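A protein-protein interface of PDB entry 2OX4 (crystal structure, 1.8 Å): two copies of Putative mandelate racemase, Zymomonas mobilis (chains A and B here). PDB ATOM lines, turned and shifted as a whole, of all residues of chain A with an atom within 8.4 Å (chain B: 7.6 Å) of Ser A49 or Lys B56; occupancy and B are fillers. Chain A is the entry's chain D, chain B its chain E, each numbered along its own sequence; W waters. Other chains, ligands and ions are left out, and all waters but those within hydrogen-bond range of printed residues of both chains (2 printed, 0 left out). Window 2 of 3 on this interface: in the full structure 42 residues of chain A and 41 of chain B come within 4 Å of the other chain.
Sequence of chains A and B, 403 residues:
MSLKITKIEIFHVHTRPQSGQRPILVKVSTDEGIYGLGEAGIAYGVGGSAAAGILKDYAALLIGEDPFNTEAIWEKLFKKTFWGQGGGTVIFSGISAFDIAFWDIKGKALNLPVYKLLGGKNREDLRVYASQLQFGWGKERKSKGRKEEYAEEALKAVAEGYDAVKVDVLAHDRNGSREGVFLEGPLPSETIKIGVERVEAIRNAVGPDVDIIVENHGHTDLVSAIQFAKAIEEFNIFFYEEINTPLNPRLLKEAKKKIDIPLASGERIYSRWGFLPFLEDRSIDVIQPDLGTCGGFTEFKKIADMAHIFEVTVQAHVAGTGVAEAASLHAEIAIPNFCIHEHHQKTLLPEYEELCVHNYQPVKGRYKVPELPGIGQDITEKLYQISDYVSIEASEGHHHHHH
NZ of Lys B56 is in hydrogen-bond range of OG of Ser A49 (2.7 Å).
The side-chain carboxylate (OD2) of Asp B57 lies within hydrogen-bond range of the backbone NH (N) of Gly A48.
The side-chain carboxylate of Asp B57 lies within hydrogen-bond range of the side-chain hydroxyl of Ser A49, at 2.6 Å.
OD2 of Asp B57 sits close to N of Gly A47.
CG1 of Val A46 touches O of Asp B57, 3.7 Å away.
Tyr B58 touches Val A46 (CD2 to CG1, 3.7 Å).
Leu B61 touches Val A46 (CD1 to CG2, 3.98 Å).
CA of Gly A47 touches CD1 of Ile B54, at 3.6 Å.
CB of Ser A49 touches O of Gly B53 (3.5 Å).
CB of Ala B50 touches O of Ala A50, at 3.4 Å.
C of Gly B53 touches N of Ala A50, 3.8 Å away.
Ala A50 touches Ile B54.
CB of Ala B50 touches CG1 of Val A90, 3.9 Å away.
CB of Val A90 touches CB of Val B90 (3.9 Å).
Ser A49 touches just these residues of chain B: Gly B53, Lys B56 and Asp B57.
Ala B51 touches none of the printed residues of chain A.
Printed residues of chain A within 4 Å of Gly B53: Ser A49 and Ala A50.
Lys B56 touches just one residue of chain A: Ser A49.
Of the printed residues of chain A, Val B90 touches Ala A50 and Val A90.
The nearest printed residue of chain A that does not touch Ala B50 is Ser A49 (5.0 Å).
Of the 21 printed residues of chain B, 9 touch a printed residue of chain A.
Hydrophobic or aromatic side chains of chain B that line the printed part of chain A: Ala B50, Ile B54, Tyr B58, Leu B61 and Val B90.
Ser A49 touches Gly B53, and with the chains exchanged Gly A53 touches Ser B49.
Ala B50 touches its own counterpart, Ala A50.
Ala A50 touches Ile B54, and with the chains exchanged Ile A54 touches Ala B50.
Val A90 touches its own counterpart, Val B90.
Positions printed for both chains: 10, 49, 50, 51, 52, 53, 54, 55, 56 and 90.
Of the 20 pairs that touch across the chains among the printed residues, 12 have their exchanged pair printed and touching as well.
Water W2 lies within hydrogen-bond range of OD1 of Asp A388 (2.6 Å), NH1 of Arg A22 (2.9 Å) and NZ of Lys B56 (2.9 Å).
Water W1 lies within hydrogen-bond range of O of Val A46 (2.8 Å) and OH of Tyr B58 (3.1 Å).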
ATOM      1  N   ILE A  10       2.467 -16.265 -34.757  1.00  0.00           N
ATOM      2  CA  ILE A  10       3.684 -17.003 -34.421  1.00  0.00           C
ATOM      3  C   ILE A  10       3.677 -18.388 -35.081  1.00  0.00           C
ATOM      4  O   ILE A  10       2.760 -19.181 -34.886  1.00  0.00           O
ATOM      5  CB  ILE A  10       3.856 -17.124 -32.886  1.00  0.00           C
ATOM      6  CG1 ILE A  10       3.832 -15.731 -32.244  1.00  0.00           C
ATOM      7  CG2 ILE A  10       5.168 -17.849 -32.554  1.00  0.00           C
ATOM      8  CD1 ILE A  10       3.297 -15.683 -30.826  1.00  0.00           C
ATOM      9  N   HIS A  12       5.691 -21.776 -35.275  1.00  0.00           N
ATOM     10  CA  HIS A  12       6.728 -22.717 -34.880  1.00  0.00           C
ATOM     11  C   HIS A  12       6.785 -23.852 -35.899  1.00  0.00           C
ATOM     12  O   HIS A  12       5.980 -24.793 -35.840  1.00  0.00           O
ATOM     13  CB  HIS A  12       6.476 -23.222 -33.448  1.00  0.00           C
ATOM     14  CG  HIS A  12       7.596 -24.046 -32.880  1.00  0.00           C
ATOM     15  ND1 HIS A  12       7.447 -24.805 -31.739  1.00  0.00           N
ATOM     16  CD2 HIS A  12       8.874 -24.240 -33.295  1.00  0.00           C
ATOM     17  CE1 HIS A  12       8.582 -25.430 -31.474  1.00  0.00           C
ATOM     18  NE2 HIS A  12       9.465 -25.104 -32.401  1.00  0.00           N
ATOM     19  N   ARG A  22      13.692 -26.714 -36.142  1.00  0.00           N
ATOM     20  CA  ARG A  22      12.353 -26.126 -36.124  1.00  0.00           C
ATOM     21  C   ARG A  22      12.453 -24.612 -35.925  1.00  0.00           C
ATOM     22  O   ARG A  22      12.472 -24.138 -34.780  1.00  0.00           O
ATOM     23  CB  ARG A  22      11.501 -26.726 -34.985  1.00  0.00           C
ATOM     24  CG  ARG A  22      11.095 -28.192 -35.180  1.00  0.00           C
ATOM     25  CD  ARG A  22       9.924 -28.608 -34.260  1.00  0.00           C
ATOM     26  NE  ARG A  22       8.705 -27.847 -34.534  1.00  0.00           N
ATOM     27  CZ  ARG A  22       7.605 -27.876 -33.787  1.00  0.00           C
ATOM     28  NH1 ARG A  22       7.551 -28.638 -32.701  1.00  0.00           N
ATOM     29  NH2 ARG A  22       6.557 -27.128 -34.115  1.00  0.00           N
ATOM     30  N   PRO A  23      12.505 -23.840 -37.031  1.00  0.00           N
ATOM     31  CA  PRO A  23      12.529 -22.369 -36.980  1.00  0.00           C
ATOM     32  C   PRO A  23      11.313 -21.788 -36.290  1.00  0.00           C
ATOM     33  O   PRO A  23      10.237 -22.407 -36.268  1.00  0.00           O
ATOM     34  CB  PRO A  23      12.502 -21.959 -38.459  1.00  0.00           C
ATOM     35  CG  PRO A  23      13.005 -23.139 -39.191  1.00  0.00           C
ATOM     36  CD  PRO A  23      12.562 -24.338 -38.417  1.00  0.00           C
ATOM     37  N   ILE A  24      11.486 -20.606 -35.711  1.00  0.00           N
ATOM     38  CA  ILE A  24      10.387 -19.883 -35.091  1.00  0.00           C
ATOM     39  C   ILE A  24      10.293 -18.483 -35.685  1.00  0.00           C
ATOM     40  O   ILE A  24      11.224 -17.691 -35.561  1.00  0.00           O
ATOM     41  CB  ILE A  24      10.521 -19.764 -33.547  1.00  0.00           C
ATOM     42  CG1 ILE A  24      10.871 -21.111 -32.904  1.00  0.00           C
ATOM     43  CG2 ILE A  24       9.209 -19.262 -32.966  1.00  0.00           C
ATOM     44  CD1 ILE A  24      12.381 -21.297 -32.602  1.00  0.00           C
ATOM     45  N   ILE A  42      16.387 -19.609 -32.064  1.00  0.00           N
ATOM     46  CA  ILE A  42      16.461 -20.904 -31.372  1.00  0.00           C
ATOM     47  C   ILE A  42      15.961 -22.036 -32.292  1.00  0.00           C
ATOM     48  O   ILE A  42      15.296 -22.967 -31.848  1.00  0.00           O
ATOM     49  CB  ILE A  42      15.645 -20.895 -30.036  1.00  0.00           C
ATOM     50  CG1 ILE A  42      15.830 -19.575 -29.279  1.00  0.00           C
ATOM     51  CG2 ILE A  42      16.044 -22.064 -29.134  1.00  0.00           C
ATOM     52  CD1 ILE A  42      15.330 -19.613 -27.848  1.00  0.00           C
ATOM     53  N   ALA A  43      16.304 -21.958 -33.578  1.00  0.00           N
ATOM     54  CA  ALA A  43      15.836 -22.943 -34.586  1.00  0.00           C
ATOM     55  C   ALA A  43      16.422 -24.339 -34.408  1.00  0.00           C
ATOM     56  O   ALA A  43      15.847 -25.322 -34.882  1.00  0.00           O
ATOM     57  CB  ALA A  43      16.114 -22.442 -36.014  1.00  0.00           C
ATOM     58  N   GLY A  45      19.006 -27.083 -31.714  1.00  0.00           N
ATOM     59  CA  GLY A  45      19.112 -27.457 -30.295  1.00  0.00           C
ATOM     60  C   GLY A  45      17.735 -27.639 -29.668  1.00  0.00           C
ATOM     61  O   GLY A  45      16.726 -27.777 -30.371  1.00  0.00           O
ATOM     62  N   VAL A  46      17.685 -27.626 -28.340  1.00  0.00           N
ATOM     63  CA  VAL A  46      16.467 -27.990 -27.621  1.00  0.00           C
ATOM     64  C   VAL A  46      15.940 -26.734 -26.924  1.00  0.00           C
ATOM     65  O   VAL A  46      16.631 -26.163 -26.071  1.00  0.00           O
ATOM     66  CB  VAL A  46      16.788 -29.086 -26.580  1.00  0.00           C
ATOM     67  CG1 VAL A  46      15.555 -29.413 -25.723  1.00  0.00           C
ATOM     68  CG2 VAL A  46      17.345 -30.330 -27.287  1.00  0.00           C
ATOM     69  N   GLY A  47      14.744 -26.285 -27.317  1.00  0.00           N
ATOM     70  CA  GLY A  47      14.124 -25.114 -26.684  1.00  0.00           C
ATOM     71  C   GLY A  47      13.242 -24.246 -27.567  1.00  0.00           C
ATOM     72  O   GLY A  47      12.707 -23.239 -27.108  1.00  0.00           O
ATOM     73  N   GLY A  48      13.055 -24.643 -28.820  1.00  0.00           N
ATOM     74  CA  GLY A  48      12.178 -23.896 -29.738  1.00  0.00           C
ATOM     75  C   GLY A  48      10.763 -23.633 -29.248  1.00  0.00           C
ATOM     76  O   GLY A  48      10.192 -22.581 -29.530  1.00  0.00           O
ATOM     77  N   SER A  49      10.174 -24.587 -28.530  1.00  0.00           N
ATOM     78  CA  SER A  49       8.826 -24.389 -28.003  1.00  0.00           C
ATOM     79  C   SER A  49       8.808 -23.295 -26.927  1.00  0.00           C
ATOM     80  O   SER A  49       7.797 -22.629 -26.733  1.00  0.00           O
ATOM     81  CB  SER A  49       8.250 -25.684 -27.425  1.00  0.00           C
ATOM     82  OG  SER A  49       8.306 -26.756 -28.361  1.00  0.00           O
ATOM     83  N   ALA A  50       9.932 -23.118 -26.233  1.00  0.00           N
ATOM     84  CA  ALA A  50      10.038 -22.018 -25.270  1.00  0.00           C
ATOM     85  C   ALA A  50      10.038 -20.659 -25.980  1.00  0.00           C
ATOM     86  O   ALA A  50       9.414 -19.724 -25.501  1.00  0.00           O
ATOM     87  CB  ALA A  50      11.276 -22.174 -24.383  1.00  0.00           C
ATOM     88  N   ALA A  51      10.749 -20.565 -27.102  1.00  0.00           N
ATOM     89  CA  ALA A  51      10.727 -19.360 -27.929  1.00  0.00           C
ATOM     90  C   ALA A  51       9.303 -19.078 -28.436  1.00  0.00           C
ATOM     91  O   ALA A  51       8.845 -17.941 -28.395  1.00  0.00           O
ATOM     92  CB  ALA A  51      11.704 -19.502 -29.099  1.00  0.00           C
ATOM     93  N   ALA A  52       8.598 -20.116 -28.895  1.00  0.00           N
ATOM     94  CA  ALA A  52       7.206 -19.922 -29.326  1.00  0.00           C
ATOM     95  C   ALA A  52       6.342 -19.392 -28.162  1.00  0.00           C
ATOM     96  O   ALA A  52       5.514 -18.492 -28.343  1.00  0.00           O
ATOM     97  CB  ALA A  52       6.624 -21.229 -29.917  1.00  0.00           C
ATOM     98  N   GLY A  53       6.575 -19.933 -26.969  1.00  0.00           N
ATOM     99  CA  GLY A  53       5.843 -19.552 -25.765  1.00  0.00           C
ATOM    100  C   GLY A  53       6.126 -18.124 -25.337  1.00  0.00           C
ATOM    101  O   GLY A  53       5.207 -17.381 -24.991  1.00  0.00           O
ATOM    102  N   ILE A  54       7.398 -17.729 -25.357  1.00  0.00           N
ATOM    103  CA  ILE A  54       7.746 -16.367 -24.929  1.00  0.00           C
ATOM    104  C   ILE A  54       7.141 -15.320 -25.867  1.00  0.00           C
ATOM    105  O   ILE A  54       6.693 -14.261 -25.407  1.00  0.00           O
ATOM    106  CB  ILE A  54       9.268 -16.147 -24.722  1.00  0.00           C
ATOM    107  CG1 ILE A  54       9.520 -14.928 -23.829  1.00  0.00           C
ATOM    108  CG2 ILE A  54      10.007 -15.933 -26.048  1.00  0.00           C
ATOM    109  CD1 ILE A  54       9.290 -15.184 -22.356  1.00  0.00           C
ATOM    110  N   LEU A  55       7.110 -15.633 -27.165  1.00  0.00           N
ATOM    111  CA  LEU A  55       6.529 -14.731 -28.162  1.00  0.00           C
ATOM    112  C   LEU A  55       5.022 -14.552 -27.894  1.00  0.00           C
ATOM    113  O   LEU A  55       4.502 -13.428 -27.897  1.00  0.00           O
ATOM    114  CB  LEU A  55       6.797 -15.265 -29.576  1.00  0.00           C
ATOM    115  CG  LEU A  55       8.258 -15.218 -30.039  1.00  0.00           C
ATOM    116  CD1 LEU A  55       8.418 -15.923 -31.382  1.00  0.00           C
ATOM    117  CD2 LEU A  55       8.781 -13.783 -30.116  1.00  0.00           C
ATOM    118  N   LYS A  56       4.340 -15.656 -27.597  1.00  0.00           N
ATOM    119  CA  LYS A  56       2.923 -15.594 -27.230  1.00  0.00           C
ATOM    120  C   LYS A  56       2.699 -14.695 -26.006  1.00  0.00           C
ATOM    121  O   LYS A  56       1.778 -13.862 -25.985  1.00  0.00           O
ATOM    122  CB  LYS A  56       2.384 -17.007 -26.979  1.00  0.00           C
ATOM    123  CG  LYS A  56       0.969 -17.015 -26.392  1.00  0.00           C
ATOM    124  CD  LYS A  56       0.265 -18.312 -26.642  1.00  0.00           C
ATOM    125  CE  LYS A  56       0.902 -19.411 -25.865  1.00  0.00           C
ATOM    126  NZ  LYS A  56       0.612 -20.718 -26.505  1.00  0.00           N
ATOM    127  N   VAL A  90      16.021 -17.482 -23.957  1.00  0.00           N
ATOM    128  CA  VAL A  90      14.640 -17.448 -24.454  1.00  0.00           C
ATOM    129  C   VAL A  90      14.080 -16.040 -24.228  1.00  0.00           C
ATOM    130  O   VAL A  90      13.439 -15.473 -25.123  1.00  0.00           O
ATOM    131  CB  VAL A  90      13.768 -18.517 -23.724  1.00  0.00           C
ATOM    132  CG1 VAL A  90      12.266 -18.413 -24.132  1.00  0.00           C
ATOM    133  CG2 VAL A  90      14.322 -19.936 -23.981  1.00  0.00           C
ATOM    134  N   ASP A 388       3.182 -25.143 -36.136  1.00  0.00           N
ATOM    135  CA  ASP A 388       2.319 -24.819 -35.000  1.00  0.00           C
ATOM    136  C   ASP A 388       2.070 -23.317 -34.985  1.00  0.00           C
ATOM    137  O   ASP A 388       3.008 -22.529 -34.841  1.00  0.00           O
ATOM    138  CB  ASP A 388       2.945 -25.249 -33.661  1.00  0.00           C
ATOM    139  CG  ASP A 388       3.205 -26.748 -33.580  1.00  0.00           C
ATOM    140  OD1 ASP A 388       4.054 -27.151 -32.755  1.00  0.00           O
ATOM    141  OD2 ASP A 388       2.562 -27.519 -34.323  1.00  0.00           O
ATOM    142  N   ILE B   8       5.528 -37.869 -18.919  1.00  0.00           N
ATOM    143  CA  ILE B   8       5.728 -36.531 -18.361  1.00  0.00           C
ATOM    144  C   ILE B   8       4.487 -35.716 -18.692  1.00  0.00           C
ATOM    145  O   ILE B   8       4.069 -35.651 -19.851  1.00  0.00           O
ATOM    146  CB  ILE B   8       7.030 -35.856 -18.920  1.00  0.00           C
ATOM    147  CG1 ILE B   8       8.279 -36.547 -18.343  1.00  0.00           C
ATOM    148  CG2 ILE B   8       7.032 -34.353 -18.597  1.00  0.00           C
ATOM    149  CD1 ILE B   8       9.594 -36.253 -19.067  1.00  0.00           C
ATOM    150  N   ILE B  10       2.607 -31.898 -18.217  1.00  0.00           N
ATOM    151  CA  ILE B  10       2.878 -30.484 -17.910  1.00  0.00           C
ATOM    152  C   ILE B  10       1.579 -29.704 -17.796  1.00  0.00           C
ATOM    153  O   ILE B  10       0.735 -29.738 -18.700  1.00  0.00           O
ATOM    154  CB  ILE B  10       3.811 -29.835 -18.966  1.00  0.00           C
ATOM    155  CG1 ILE B  10       5.088 -30.659 -19.101  1.00  0.00           C
ATOM    156  CG2 ILE B  10       4.162 -28.370 -18.570  1.00  0.00           C
ATOM    157  CD1 ILE B  10       5.676 -30.646 -20.468  1.00  0.00           C
ATOM    158  N   VAL B  26       4.914 -29.814 -13.260  1.00  0.00           N
ATOM    159  CA  VAL B  26       5.282 -30.991 -14.013  1.00  0.00           C
ATOM    160  C   VAL B  26       5.066 -32.261 -13.168  1.00  0.00           C
ATOM    161  O   VAL B  26       5.434 -32.312 -11.997  1.00  0.00           O
ATOM    162  CB  VAL B  26       6.731 -30.874 -14.619  1.00  0.00           C
ATOM    163  CG1 VAL B  26       7.832 -30.884 -13.512  1.00  0.00           C
ATOM    164  CG2 VAL B  26       6.979 -31.983 -15.645  1.00  0.00           C
ATOM    165  N   SER B  49       4.327 -19.168 -20.460  1.00  0.00           N
ATOM    166  CA  SER B  49       4.163 -20.054 -21.614  1.00  0.00           C
ATOM    167  C   SER B  49       5.515 -20.550 -22.115  1.00  0.00           C
ATOM    168  O   SER B  49       5.620 -21.650 -22.643  1.00  0.00           O
ATOM    169  CB  SER B  49       3.422 -19.361 -22.767  1.00  0.00           C
ATOM    170  OG  SER B  49       2.158 -18.908 -22.352  1.00  0.00           O
ATOM    171  N   ALA B  50       6.553 -19.728 -21.950  1.00  0.00           N
ATOM    172  CA  ALA B  50       7.905 -20.166 -22.287  1.00  0.00           C
ATOM    173  C   ALA B  50       8.363 -21.316 -21.376  1.00  0.00           C
ATOM    174  O   ALA B  50       8.965 -22.280 -21.855  1.00  0.00           O
ATOM    175  CB  ALA B  50       8.879 -19.009 -22.210  1.00  0.00           C
ATOM    176  N   ALA B  51       8.079 -21.196 -20.077  1.00  0.00           N
ATOM    177  CA  ALA B  51       8.302 -22.294 -19.124  1.00  0.00           C
ATOM    178  C   ALA B  51       7.582 -23.575 -19.535  1.00  0.00           C
ATOM    179  O   ALA B  51       8.181 -24.659 -19.534  1.00  0.00           O
ATOM    180  CB  ALA B  51       7.900 -21.879 -17.702  1.00  0.00           C
ATOM    181  N   ALA B  52       6.300 -23.471 -19.885  1.00  0.00           N
ATOM    182  CA  ALA B  52       5.581 -24.657 -20.375  1.00  0.00           C
ATOM    183  C   ALA B  52       6.270 -25.289 -21.602  1.00  0.00           C
ATOM    184  O   ALA B  52       6.420 -26.512 -21.678  1.00  0.00           O
ATOM    185  CB  ALA B  52       4.116 -24.317 -20.662  1.00  0.00           C
ATOM    186  N   GLY B  53       6.727 -24.435 -22.527  1.00  0.00           N
ATOM    187  CA  GLY B  53       7.409 -24.858 -23.747  1.00  0.00           C
ATOM    188  C   GLY B  53       8.755 -25.524 -23.510  1.00  0.00           C
ATOM    189  O   GLY B  53       9.065 -26.539 -24.132  1.00  0.00           O
ATOM    190  N   ILE B  54       9.565 -24.964 -22.609  1.00  0.00           N
ATOM    191  CA  ILE B  54      10.858 -25.578 -22.313  1.00  0.00           C
ATOM    192  C   ILE B  54      10.719 -26.971 -21.684  1.00  0.00           C
ATOM    193  O   ILE B  54      11.513 -27.868 -21.977  1.00  0.00           O
ATOM    194  CB  ILE B  54      11.808 -24.653 -21.486  1.00  0.00           C
ATOM    195  CG1 ILE B  54      13.271 -25.061 -21.681  1.00  0.00           C
ATOM    196  CG2 ILE B  54      11.461 -24.667 -19.990  1.00  0.00           C
ATOM    197  CD1 ILE B  54      13.826 -24.789 -23.068  1.00  0.00           C
ATOM    198  N   LEU B  55       9.716 -27.144 -20.822  1.00  0.00           N
ATOM    199  CA  LEU B  55       9.450 -28.443 -20.209  1.00  0.00           C
ATOM    200  C   LEU B  55       9.053 -29.483 -21.261  1.00  0.00           C
ATOM    201  O   LEU B  55       9.500 -30.629 -21.210  1.00  0.00           O
ATOM    202  CB  LEU B  55       8.366 -28.330 -19.126  1.00  0.00           C
ATOM    203  CG  LEU B  55       8.714 -27.445 -17.915  1.00  0.00           C
ATOM    204  CD1 LEU B  55       7.510 -27.272 -17.029  1.00  0.00           C
ATOM    205  CD2 LEU B  55       9.877 -28.055 -17.130  1.00  0.00           C
ATOM    206  N   LYS B  56       8.234 -29.059 -22.221  1.00  0.00           N
ATOM    207  CA  LYS B  56       7.815 -29.913 -23.325  1.00  0.00           C
ATOM    208  C   LYS B  56       9.035 -30.360 -24.145  1.00  0.00           C
ATOM    209  O   LYS B  56       9.197 -31.551 -24.457  1.00  0.00           O
ATOM    210  CB  LYS B  56       6.777 -29.165 -24.181  1.00  0.00           C
ATOM    211  CG  LYS B  56       6.407 -29.843 -25.502  1.00  0.00           C
ATOM    212  CD  LYS B  56       5.407 -28.967 -26.264  1.00  0.00           C
ATOM    213  CE  LYS B  56       5.340 -29.340 -27.743  1.00  0.00           C
ATOM    214  NZ  LYS B  56       6.168 -28.458 -28.626  1.00  0.00           N
ATOM    215  N   ASP B  57       9.923 -29.419 -24.446  1.00  0.00           N
ATOM    216  CA  ASP B  57      11.118 -29.734 -25.205  1.00  0.00           C
ATOM    217  C   ASP B  57      12.076 -30.642 -24.450  1.00  0.00           C
ATOM    218  O   ASP B  57      12.619 -31.588 -25.025  1.00  0.00           O
ATOM    219  CB  ASP B  57      11.828 -28.454 -25.636  1.00  0.00           C
ATOM    220  CG  ASP B  57      11.070 -27.708 -26.711  1.00  0.00           C
ATOM    221  OD1 ASP B  57      10.163 -28.301 -27.347  1.00  0.00           O
ATOM    222  OD2 ASP B  57      11.375 -26.520 -26.917  1.00  0.00           O
ATOM    223  N   TYR B  58      12.295 -30.346 -23.168  1.00  0.00           N
ATOM    224  CA  TYR B  58      13.214 -31.135 -22.355  1.00  0.00           C
ATOM    225  C   TYR B  58      12.693 -32.563 -22.143  1.00  0.00           C
ATOM    226  O   TYR B  58      13.491 -33.501 -22.014  1.00  0.00           O
ATOM    227  CB  TYR B  58      13.440 -30.473 -20.986  1.00  0.00           C
ATOM    228  CG  TYR B  58      14.355 -29.260 -20.965  1.00  0.00           C
ATOM    229  CD1 TYR B  58      14.560 -28.557 -19.769  1.00  0.00           C
ATOM    230  CD2 TYR B  58      15.007 -28.807 -22.110  1.00  0.00           C
ATOM    231  CE1 TYR B  58      15.396 -27.442 -19.712  1.00  0.00           C
ATOM    232  CE2 TYR B  58      15.843 -27.671 -22.068  1.00  0.00           C
ATOM    233  CZ  TYR B  58      16.035 -27.006 -20.862  1.00  0.00           C
ATOM    234  OH  TYR B  58      16.837 -25.893 -20.785  1.00  0.00           O
ATOM    235  N   ALA B  59      11.366 -32.705 -22.106  1.00  0.00           N
ATOM    236  CA  ALA B  59      10.703 -33.995 -21.855  1.00  0.00           C
ATOM    237  C   ALA B  59      11.172 -35.108 -22.800  1.00  0.00           C
ATOM    238  O   ALA B  59      11.353 -36.261 -22.375  1.00  0.00           O
ATOM    239  CB  ALA B  59       9.199 -33.835 -21.935  1.00  0.00           C
ATOM    240  N   ALA B  60      11.397 -34.745 -24.065  1.00  0.00           N
ATOM    241  CA  ALA B  60      11.880 -35.682 -25.083  1.00  0.00           C
ATOM    242  C   ALA B  60      13.214 -36.323 -24.725  1.00  0.00           C
ATOM    243  O   ALA B  60      13.467 -37.474 -25.080  1.00  0.00           O
ATOM    244  CB  ALA B  60      11.985 -34.986 -26.427  1.00  0.00           C
ATOM    245  N   LEU B  61      14.067 -35.580 -24.023  1.00  0.00           N
ATOM    246  CA  LEU B  61      15.374 -36.084 -23.619  1.00  0.00           C
ATOM    247  C   LEU B  61      15.275 -36.957 -22.374  1.00  0.00           C
ATOM    248  O   LEU B  61      16.235 -37.634 -22.011  1.00  0.00           O
ATOM    249  CB  LEU B  61      16.343 -34.931 -23.371  1.00  0.00           C
ATOM    250  CG  LEU B  61      16.960 -34.168 -24.560  1.00  0.00           C
ATOM    251  CD1 LEU B  61      15.909 -33.572 -25.473  1.00  0.00           C
ATOM    252  CD2 LEU B  61      17.872 -33.071 -24.034  1.00  0.00           C
ATOM    253  N   VAL B  90      14.377 -19.039 -18.351  1.00  0.00           N
ATOM    254  CA  VAL B  90      13.491 -20.113 -18.811  1.00  0.00           C
ATOM    255  C   VAL B  90      14.292 -21.413 -18.920  1.00  0.00           C
ATOM    256  O   VAL B  90      13.836 -22.471 -18.470  1.00  0.00           O
ATOM    257  CB  VAL B  90      12.826 -19.755 -20.175  1.00  0.00           C
ATOM    258  CG1 VAL B  90      11.912 -20.909 -20.663  1.00  0.00           C
ATOM    259  CG2 VAL B  90      12.010 -18.453 -20.061  1.00  0.00           C
ATOM    260  N   PHE B  98      12.022 -30.272 -13.396  1.00  0.00           N
ATOM    261  CA  PHE B  98      12.294 -31.698 -13.511  1.00  0.00           C
ATOM    262  C   PHE B  98      13.133 -32.218 -12.359  1.00  0.00           C
ATOM    263  O   PHE B  98      12.854 -33.284 -11.829  1.00  0.00           O
ATOM    264  CB  PHE B  98      12.971 -32.017 -14.839  1.00  0.00           C
ATOM    265  CG  PHE B  98      12.016 -32.061 -15.996  1.00  0.00           C
ATOM    266  CD1 PHE B  98      12.114 -31.137 -17.032  1.00  0.00           C
ATOM    267  CD2 PHE B  98      11.008 -33.027 -16.043  1.00  0.00           C
ATOM    268  CE1 PHE B  98      11.218 -31.164 -18.106  1.00  0.00           C
ATOM    269  CE2 PHE B  98      10.112 -33.078 -17.117  1.00  0.00           C
ATOM    270  CZ  PHE B  98      10.212 -32.141 -18.152  1.00  0.00           C
ATOM    271  N   VAL B 390      -0.276 -30.759 -21.321  1.00  0.00           N
ATOM    272  CA  VAL B 390       0.537 -31.450 -22.321  1.00  0.00           C
ATOM    273  C   VAL B 390       1.060 -32.765 -21.723  1.00  0.00           C
ATOM    274  O   VAL B 390       1.602 -32.778 -20.616  1.00  0.00           O
ATOM    275  CB  VAL B 390       1.720 -30.552 -22.827  1.00  0.00           C
ATOM    276  CG1 VAL B 390       2.692 -31.345 -23.668  1.00  0.00           C
ATOM    277  CG2 VAL B 390       1.194 -29.367 -23.654  1.00  0.00           C
ATOM    278  N   SER B 391       0.890 -33.869 -22.447  1.00  0.00           N
ATOM    279  CA  SER B 391       1.455 -35.158 -22.024  1.00  0.00           C
ATOM    280  C   SER B 391       2.479 -35.683 -23.021  1.00  0.00           C
ATOM    281  O   SER B 391       2.262 -35.627 -24.230  1.00  0.00           O
ATOM    282  CB  SER B 391       0.340 -36.189 -21.823  1.00  0.00           C
ATOM    283  OG  SER B 391       0.863 -37.432 -21.403  1.00  0.00           O
ATOM    284  N   ILE B 392       3.600 -36.185 -22.511  1.00  0.00           N
ATOM    285  CA  ILE B 392       4.673 -36.732 -23.349  1.00  0.00           C
ATOM    286  C   ILE B 392       4.987 -38.154 -22.882  1.00  0.00           C
ATOM    287  O   ILE B 392       5.214 -38.386 -21.697  1.00  0.00           O
ATOM    288  CB  ILE B 392       5.964 -35.855 -23.300  1.00  0.00           C
ATOM    289  CG1 ILE B 392       5.692 -34.446 -23.841  1.00  0.00           C
ATOM    290  CG2 ILE B 392       7.072 -36.456 -24.153  1.00  0.00           C
ATOM    291  CD1 ILE B 392       5.608 -33.407 -22.788  1.00  0.00           C
HETATM  292  O   HOH W   1      17.956 -25.655 -23.656  1.00  0.00           O
HETATM  293  O   HOH W   2       5.112 -28.957 -31.255  1.00  0.00           O
